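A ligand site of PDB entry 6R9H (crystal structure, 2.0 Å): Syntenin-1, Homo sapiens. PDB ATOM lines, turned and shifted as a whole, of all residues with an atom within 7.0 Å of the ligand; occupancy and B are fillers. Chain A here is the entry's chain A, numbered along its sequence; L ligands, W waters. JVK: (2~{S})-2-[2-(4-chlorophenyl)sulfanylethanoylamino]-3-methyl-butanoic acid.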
ATOM      1  N   LYS A  96     -29.895 -21.239  11.954  1.00  0.00           N
ATOM      2  CA  LYS A  96     -28.912 -22.220  11.438  1.00  0.00           C
ATOM      3  C   LYS A  96     -28.749 -23.343  12.468  1.00  0.00           C
ATOM      4  O   LYS A  96     -28.748 -23.056  13.695  1.00  0.00           O
ATOM      5  CB  LYS A  96     -27.560 -21.551  11.177  1.00  0.00           C
ATOM      6  CG  LYS A  96     -27.537 -20.551  10.050  1.00  0.00           C
ATOM      7  CD  LYS A  96     -26.168 -19.994   9.779  1.00  0.00           C
ATOM      8  CE  LYS A  96     -26.054 -19.388   8.401  1.00  0.00           C
ATOM      9  NZ  LYS A  96     -24.694 -18.860   8.129  1.00  0.00           N
ATOM     10  N   GLY A 100     -24.547 -25.163  10.234  1.00  0.00           N
ATOM     11  CA  GLY A 100     -24.692 -23.849   9.594  1.00  0.00           C
ATOM     12  C   GLY A 100     -25.769 -23.807   8.516  1.00  0.00           C
ATOM     13  O   GLY A 100     -25.773 -22.821   7.723  1.00  0.00           O
ATOM     14  N   HIS A 101     -26.672 -24.787   8.460  1.00  0.00           N
ATOM     15  CA  HIS A 101     -27.770 -24.858   7.457  1.00  0.00           C
ATOM     16  C   HIS A 101     -29.124 -24.447   8.066  1.00  0.00           C
ATOM     17  O   HIS A 101     -29.371 -24.768   9.247  1.00  0.00           O
ATOM     18  CB  HIS A 101     -27.838 -26.263   6.839  1.00  0.00           C
ATOM     19  CG  HIS A 101     -26.613 -26.614   6.083  1.00  0.00           C
ATOM     20  ND1 HIS A 101     -25.590 -27.384   6.617  1.00  0.00           N
ATOM     21  CD2 HIS A 101     -26.197 -26.243   4.842  1.00  0.00           C
ATOM     22  CE1 HIS A 101     -24.606 -27.477   5.739  1.00  0.00           C
ATOM     23  NE2 HIS A 101     -24.964 -26.799   4.623  1.00  0.00           N
ATOM     24  N   VAL A 102     -29.966 -23.788   7.279  1.00  0.00           N
ATOM     25  CA  VAL A 102     -31.394 -23.516   7.618  1.00  0.00           C
ATOM     26  C   VAL A 102     -32.326 -24.583   7.014  1.00  0.00           C
ATOM     27  O   VAL A 102     -33.410 -24.797   7.571  1.00  0.00           O
ATOM     28  CB  VAL A 102     -31.801 -22.075   7.238  1.00  0.00           C
ATOM     29  CG1 VAL A 102     -31.050 -21.092   8.131  1.00  0.00           C
ATOM     30  CG2 VAL A 102     -31.608 -21.757   5.785  1.00  0.00           C
ATOM     31  N   GLY A 103     -31.930 -25.210   5.901  1.00  0.00           N
ATOM     32  CA  GLY A 103     -32.591 -26.421   5.343  1.00  0.00           C
ATOM     33  C   GLY A 103     -33.436 -26.173   4.091  1.00  0.00           C
ATOM     34  O   GLY A 103     -34.597 -26.630   4.055  1.00  0.00           O
ATOM     35  N   PHE A 104     -32.895 -25.527   3.063  1.00  0.00           N
ATOM     36  CA  PHE A 104     -33.565 -25.456   1.749  1.00  0.00           C
ATOM     37  C   PHE A 104     -32.558 -25.484   0.598  1.00  0.00           C
ATOM     38  O   PHE A 104     -31.398 -25.116   0.779  1.00  0.00           O
ATOM     39  CB  PHE A 104     -34.506 -24.258   1.605  1.00  0.00           C
ATOM     40  CG  PHE A 104     -33.869 -22.893   1.631  1.00  0.00           C
ATOM     41  CD1 PHE A 104     -33.764 -22.184   2.811  1.00  0.00           C
ATOM     42  CD2 PHE A 104     -33.479 -22.274   0.468  1.00  0.00           C
ATOM     43  CE1 PHE A 104     -33.224 -20.903   2.826  1.00  0.00           C
ATOM     44  CE2 PHE A 104     -32.898 -21.011   0.481  1.00  0.00           C
ATOM     45  CZ  PHE A 104     -32.780 -20.330   1.658  1.00  0.00           C
ATOM     46  N   ILE A 105     -33.061 -25.949  -0.544  1.00  0.00           N
ATOM     47  CA  ILE A 105     -32.407 -25.976  -1.874  1.00  0.00           C
ATOM     48  C   ILE A 105     -33.074 -24.878  -2.701  1.00  0.00           C
ATOM     49  O   ILE A 105     -34.309 -24.662  -2.585  1.00  0.00           O
ATOM     50  CB  ILE A 105     -32.575 -27.362  -2.538  1.00  0.00           C
ATOM     51  CG1 ILE A 105     -32.250 -28.526  -1.594  1.00  0.00           C
ATOM     52  CG2 ILE A 105     -31.789 -27.434  -3.827  1.00  0.00           C
ATOM     53  CD1 ILE A 105     -30.912 -28.435  -0.923  1.00  0.00           C
ATOM     54  N   PHE A 106     -32.301 -24.218  -3.550  1.00  0.00           N
ATOM     55  CA  PHE A 106     -32.839 -23.230  -4.507  1.00  0.00           C
ATOM     56  C   PHE A 106     -32.075 -23.337  -5.818  1.00  0.00           C
ATOM     57  O   PHE A 106     -30.954 -23.872  -5.844  1.00  0.00           O
ATOM     58  CB  PHE A 106     -32.783 -21.824  -3.902  1.00  0.00           C
ATOM     59  CG  PHE A 106     -31.393 -21.319  -3.678  1.00  0.00           C
ATOM     60  CD1 PHE A 106     -30.699 -21.680  -2.538  1.00  0.00           C
ATOM     61  CD2 PHE A 106     -30.805 -20.454  -4.569  1.00  0.00           C
ATOM     62  CE1 PHE A 106     -29.427 -21.197  -2.296  1.00  0.00           C
ATOM     63  CE2 PHE A 106     -29.524 -19.983  -4.344  1.00  0.00           C
ATOM     64  CZ  PHE A 106     -28.840 -20.366  -3.211  1.00  0.00           C
ATOM     65  N   LYS A 107     -32.686 -22.807  -6.873  1.00  0.00           N
ATOM     66  CA  LYS A 107     -32.117 -22.729  -8.246  1.00  0.00           C
ATOM     67  C   LYS A 107     -32.698 -21.489  -8.913  1.00  0.00           C
ATOM     68  O   LYS A 107     -33.919 -21.297  -8.844  1.00  0.00           O
ATOM     69  CB  LYS A 107     -32.444 -23.969  -9.076  1.00  0.00           C
ATOM     70  CG  LYS A 107     -31.732 -23.998 -10.422  1.00  0.00           C
ATOM     71  CD  LYS A 107     -32.355 -24.954 -11.392  1.00  0.00           C
ATOM     72  CE  LYS A 107     -31.512 -25.161 -12.635  1.00  0.00           C
ATOM     73  NZ  LYS A 107     -32.093 -26.239 -13.462  1.00  0.00           N
ATOM     74  N   ASN A 108     -31.824 -20.673  -9.495  1.00  0.00           N
ATOM     75  CA  ASN A 108     -32.161 -19.378 -10.141  1.00  0.00           C
ATOM     76  C   ASN A 108     -32.918 -18.507  -9.138  1.00  0.00           C
ATOM     77  O   ASN A 108     -33.924 -17.905  -9.514  1.00  0.00           O
ATOM     78  CB  ASN A 108     -32.921 -19.618 -11.455  1.00  0.00           C
ATOM     79  CG  ASN A 108     -32.100 -20.459 -12.423  1.00  0.00           C
ATOM     80  OD1 ASN A 108     -32.533 -21.508 -12.877  1.00  0.00           O
ATOM     81  ND2 ASN A 108     -30.878 -20.050 -12.724  1.00  0.00           N
ATOM     82  N   THR A 112     -36.626 -24.530  -4.208  1.00  0.00           N
ATOM     83  CA  THR A 112     -37.105 -25.715  -4.951  1.00  0.00           C
ATOM     84  C   THR A 112     -37.409 -26.887  -4.006  1.00  0.00           C
ATOM     85  O   THR A 112     -38.215 -27.734  -4.414  1.00  0.00           O
ATOM     86  CB  THR A 112     -36.100 -26.138  -6.035  1.00  0.00           C
ATOM     87  OG1 THR A 112     -34.855 -26.356  -5.392  1.00  0.00           O
ATOM     88  CG2 THR A 112     -35.972 -25.126  -7.142  1.00  0.00           C
ATOM     89  N   VAL A 115     -35.699 -29.140   3.330  1.00  0.00           N
ATOM     90  CA  VAL A 115     -35.035 -30.310   3.980  1.00  0.00           C
ATOM     91  C   VAL A 115     -35.846 -30.683   5.222  1.00  0.00           C
ATOM     92  O   VAL A 115     -36.187 -29.773   6.044  1.00  0.00           O
ATOM     93  CB  VAL A 115     -33.569 -29.990   4.280  1.00  0.00           C
ATOM     94  CG1 VAL A 115     -32.848 -31.132   4.981  1.00  0.00           C
ATOM     95  CG2 VAL A 115     -32.821 -29.599   3.029  1.00  0.00           C
ATOM     96  N   SER A 118     -35.593 -29.498   9.406  1.00  0.00           N
ATOM     97  CA  SER A 118     -34.766 -28.266   9.356  1.00  0.00           C
ATOM     98  C   SER A 118     -35.559 -27.087   9.948  1.00  0.00           C
ATOM     99  O   SER A 118     -36.786 -27.186  10.098  1.00  0.00           O
ATOM    100  CB  SER A 118     -34.372 -27.967   7.941  1.00  0.00           C
ATOM    101  OG  SER A 118     -35.516 -27.577   7.178  1.00  0.00           O
ATOM    102  N   ALA A 120     -36.137 -24.480   8.247  1.00  0.00           N
ATOM    103  CA  ALA A 120     -37.006 -24.134   7.085  1.00  0.00           C
ATOM    104  C   ALA A 120     -38.321 -24.911   7.210  1.00  0.00           C
ATOM    105  O   ALA A 120     -39.387 -24.314   7.031  1.00  0.00           O
ATOM    106  CB  ALA A 120     -36.292 -24.421   5.763  1.00  0.00           C
ATOM    107  N   ILE A 131     -36.333 -15.738  -3.749  1.00  0.00           N
ATOM    108  CA  ILE A 131     -35.638 -15.091  -2.597  1.00  0.00           C
ATOM    109  C   ILE A 131     -35.390 -13.638  -2.997  1.00  0.00           C
ATOM    110  O   ILE A 131     -34.748 -13.439  -4.043  1.00  0.00           O
ATOM    111  CB  ILE A 131     -34.324 -15.821  -2.259  1.00  0.00           C
ATOM    112  CG1 ILE A 131     -34.522 -17.334  -2.145  1.00  0.00           C
ATOM    113  CG2 ILE A 131     -33.752 -15.211  -0.996  1.00  0.00           C
ATOM    114  CD1 ILE A 131     -33.247 -18.137  -2.085  1.00  0.00           C
ATOM    115  N   LYS A 143     -26.219 -14.393  -8.685  1.00  0.00           N
ATOM    116  CA  LYS A 143     -26.030 -15.806  -9.094  1.00  0.00           C
ATOM    117  C   LYS A 143     -26.288 -16.652  -7.839  1.00  0.00           C
ATOM    118  O   LYS A 143     -26.057 -16.150  -6.729  1.00  0.00           O
ATOM    119  CB  LYS A 143     -24.621 -16.040  -9.663  1.00  0.00           C
ATOM    120  CG  LYS A 143     -24.116 -15.027 -10.689  1.00  0.00           C
ATOM    121  CD  LYS A 143     -24.866 -15.076 -11.984  1.00  0.00           C
ATOM    122  CE  LYS A 143     -26.083 -14.174 -12.082  1.00  0.00           C
ATOM    123  NZ  LYS A 143     -26.617 -14.175 -13.467  1.00  0.00           N
ATOM    124  N   ASP A 144     -26.737 -17.893  -8.031  1.00  0.00           N
ATOM    125  CA  ASP A 144     -27.001 -18.868  -6.942  1.00  0.00           C
ATOM    126  C   ASP A 144     -25.792 -18.955  -6.011  1.00  0.00           C
ATOM    127  O   ASP A 144     -26.020 -19.029  -4.793  1.00  0.00           O
ATOM    128  CB  ASP A 144     -27.412 -20.219  -7.521  1.00  0.00           C
ATOM    129  CG  ASP A 144     -28.810 -20.148  -8.113  1.00  0.00           C
ATOM    130  OD1 ASP A 144     -29.529 -19.165  -7.784  1.00  0.00           O
ATOM    131  OD2 ASP A 144     -29.155 -21.033  -8.958  1.00  0.00           O
ATOM    132  N   SER A 145     -24.555 -18.961  -6.536  1.00  0.00           N
ATOM    133  CA  SER A 145     -23.350 -19.176  -5.692  1.00  0.00           C
ATOM    134  C   SER A 145     -23.160 -17.952  -4.770  1.00  0.00           C
ATOM    135  O   SER A 145     -22.765 -18.124  -3.633  1.00  0.00           O
ATOM    136  CB  SER A 145     -22.113 -19.550  -6.509  1.00  0.00           C
ATOM    137  OG  SER A 145     -21.575 -18.432  -7.217  1.00  0.00           O
ATOM    138  N   GLN A 146     -23.524 -16.770  -5.247  1.00  0.00           N
ATOM    139  CA  GLN A 146     -23.450 -15.499  -4.460  1.00  0.00           C
ATOM    140  C   GLN A 146     -24.510 -15.508  -3.339  1.00  0.00           C
ATOM    141  O   GLN A 146     -24.209 -15.016  -2.241  1.00  0.00           O
ATOM    142  CB  GLN A 146     -23.661 -14.282  -5.368  1.00  0.00           C
ATOM    143  CG  GLN A 146     -22.570 -14.107  -6.411  1.00  0.00           C
ATOM    144  CD  GLN A 146     -22.812 -12.882  -7.256  1.00  0.00           C
ATOM    145  OE1 GLN A 146     -23.742 -12.819  -8.033  1.00  0.00           O
ATOM    146  NE2 GLN A 146     -21.973 -11.880  -7.080  1.00  0.00           N
ATOM    147  N   ILE A 147     -25.692 -16.054  -3.615  1.00  0.00           N
ATOM    148  CA  ILE A 147     -26.766 -16.213  -2.588  1.00  0.00           C
ATOM    149  C   ILE A 147     -26.261 -17.185  -1.510  1.00  0.00           C
ATOM    150  O   ILE A 147     -26.331 -16.835  -0.318  1.00  0.00           O
ATOM    151  CB  ILE A 147     -28.099 -16.624  -3.246  1.00  0.00           C
ATOM    152  CG1 ILE A 147     -28.592 -15.548  -4.204  1.00  0.00           C
ATOM    153  CG2 ILE A 147     -29.146 -16.947  -2.185  1.00  0.00           C
ATOM    154  CD1 ILE A 147     -29.879 -15.867  -4.907  1.00  0.00           C
ATOM    155  N   ALA A 148     -25.696 -18.320  -1.918  1.00  0.00           N
ATOM    156  CA  ALA A 148     -25.062 -19.294  -0.983  1.00  0.00           C
ATOM    157  C   ALA A 148     -23.958 -18.596  -0.167  1.00  0.00           C
ATOM    158  O   ALA A 148     -23.898 -18.866   1.047  1.00  0.00           O
ATOM    159  CB  ALA A 148     -24.539 -20.488  -1.747  1.00  0.00           C
ATOM    160  N   ASP A 149     -23.133 -17.745  -0.789  1.00  0.00           N
ATOM    161  CA  ASP A 149     -22.054 -17.021  -0.061  1.00  0.00           C
ATOM    162  C   ASP A 149     -22.656 -16.179   1.073  1.00  0.00           C
ATOM    163  O   ASP A 149     -22.122 -16.168   2.142  1.00  0.00           O
ATOM    164  CB  ASP A 149     -21.221 -16.130  -0.997  1.00  0.00           C
ATOM    165  CG  ASP A 149     -20.348 -16.896  -1.983  1.00  0.00           C
ATOM    166  OD1 ASP A 149     -20.016 -18.078  -1.702  1.00  0.00           O
ATOM    167  OD2 ASP A 149     -20.049 -16.326  -3.041  1.00  0.00           O
ATOM    168  N   LEU A 151     -25.651 -16.553   2.563  1.00  0.00           N
ATOM    169  CA  LEU A 151     -26.234 -17.457   3.595  1.00  0.00           C
ATOM    170  C   LEU A 151     -25.095 -18.032   4.439  1.00  0.00           C
ATOM    171  O   LEU A 151     -25.243 -18.066   5.667  1.00  0.00           O
ATOM    172  CB  LEU A 151     -27.083 -18.557   2.932  1.00  0.00           C
ATOM    173  CG  LEU A 151     -28.409 -18.050   2.351  1.00  0.00           C
ATOM    174  CD1 LEU A 151     -28.912 -18.921   1.217  1.00  0.00           C
ATOM    175  CD2 LEU A 151     -29.453 -17.921   3.442  1.00  0.00           C
ATOM    176  N   SER A 152     -23.978 -18.421   3.820  1.00  0.00           N
ATOM    177  CA  SER A 152     -22.853 -19.065   4.539  1.00  0.00           C
ATOM    178  C   SER A 152     -22.203 -18.065   5.508  1.00  0.00           C
ATOM    179  O   SER A 152     -21.722 -18.502   6.548  1.00  0.00           O
ATOM    180  CB  SER A 152     -21.878 -19.687   3.619  1.00  0.00           C
ATOM    181  OG  SER A 152     -21.149 -20.672   4.315  1.00  0.00           O
ATOM    182  N   VAL A 158     -31.373 -16.119  10.330  1.00  0.00           N
ATOM    183  CA  VAL A 158     -31.512 -15.890   8.853  1.00  0.00           C
ATOM    184  C   VAL A 158     -32.973 -15.501   8.587  1.00  0.00           C
ATOM    185  O   VAL A 158     -33.843 -16.353   8.735  1.00  0.00           O
ATOM    186  CB  VAL A 158     -31.105 -17.137   8.040  1.00  0.00           C
ATOM    187  CG1 VAL A 158     -31.246 -16.887   6.557  1.00  0.00           C
ATOM    188  CG2 VAL A 158     -29.691 -17.591   8.366  1.00  0.00           C
HETATM  189  C   JVK L   1     -26.716 -23.800  -2.575  1.00  0.00           C
HETATM  190  N   JVK L   1     -28.723 -24.563   1.450  1.00  0.00           N
HETATM  191  S   JVK L   1     -29.161 -24.920  -1.922  1.00  0.00           S
HETATM  192  C1  JVK L   1     -27.955 -24.189  -3.074  1.00  0.00           C
HETATM  193  C2  JVK L   1     -28.293 -24.017  -4.429  1.00  0.00           C
HETATM  194  C3  JVK L   1     -27.387 -23.461  -5.307  1.00  0.00           C
HETATM  195  C4  JVK L   1     -26.146 -23.072  -4.794  1.00  0.00           C
HETATM  196  C5  JVK L   1     -25.798 -23.236  -3.447  1.00  0.00           C
HETATM  197  C6  JVK L   1     -28.553 -26.048  -0.584  1.00  0.00           C
HETATM  198  C7  JVK L   1     -27.882 -25.372   0.624  1.00  0.00           C
HETATM  199  C8  JVK L   1     -28.254 -23.793   2.582  1.00  0.00           C
HETATM  200  C9  JVK L   1     -29.086 -23.984   3.840  1.00  0.00           C
HETATM  201  C10 JVK L   1     -28.385 -22.375   2.077  1.00  0.00           C
HETATM  202  C11 JVK L   1     -27.457 -22.139   0.864  1.00  0.00           C
HETATM  203  C12 JVK L   1     -29.824 -22.038   1.668  1.00  0.00           C
HETATM  204  O   JVK L   1     -26.719 -25.524   0.912  1.00  0.00           O
HETATM  205 CL   JVK L   1     -24.896 -22.343  -5.802  1.00  0.00          CL
HETATM  206  O1  JVK L   1     -28.829 -23.192   4.800  1.00  0.00           O
HETATM  207  O2  JVK L   1     -29.914 -24.927   3.824  1.00  0.00           O
HETATM  208  O   HOH W   1     -26.901 -21.669   5.230  1.00  0.00           O
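N of Phe 104 sits at hydrogen-bond distance from O2 of the ligand (3.1 Å). The backbone carbonyl oxygen (O) of Phe 104 sits at hydrogen-bond distance from a nitrogen (N) of the ligand (2.8 Å). N of Val 102 lies within hydrogen-bond range of O1 of the ligand, at 2.8 Å. A sulfur (S) of the ligand sits close to the backbone NH (N) of Phe 106. The backbone NH (N) of Gly 103 sits at hydrogen-bond distance from an oxygen (O2) of the ligand (2.9 Å).
The backbone NH (N) of Ala 120 lies within hydrogen-bond range of the backbone carbonyl oxygen (O) of Val 102 (2.8 Å). NZ of Lys 96 lies within hydrogen-bond range of O of Leu 151 (2.6 Å). N of Thr 112 is in hydrogen-bond range of O of Ile 105, at 2.8 Å. OD2 of Asp 144 is in hydrogen-bond range of N of Asn 108, 2.7 Å away. O of Gly 103 is in hydrogen-bond range of N of Val 115 (2.8 Å). The side-chain hydroxyl (OG) of Ser 118 is in hydrogen-bond range of the backbone carbonyl oxygen (O) of Gly 103 (3.4 Å).
His 101 touches the ligand (CA to O1, 3.3 Å). Ile 105 touches the ligand (CD1 to C6, 3.4 Å). C of Asp 144 touches CL of the ligand (3.5 Å). N of Ser 145 touches CL of the ligand, at 3.5 Å. Ala 148 touches the ligand. Leu 151 touches the ligand. Hydrophobic or aromatic side chains that line the ligand: His 101, Val 102, Phe 104, Ile 105, Phe 106, Ala 148 and Leu 151. Within 4 Å of the ligand: His 101, Val 102, Gly 103, Phe 104, Ile 105, Phe 106, Asp 144, Ser 145, Ala 148 and Leu 151. The nearest printed residue that does not touch the ligand is Gly 100 (4.2 Å).
Water W1 bridges an oxygen (O1) of the ligand and the backbone carbonyl oxygen of Gly 100.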
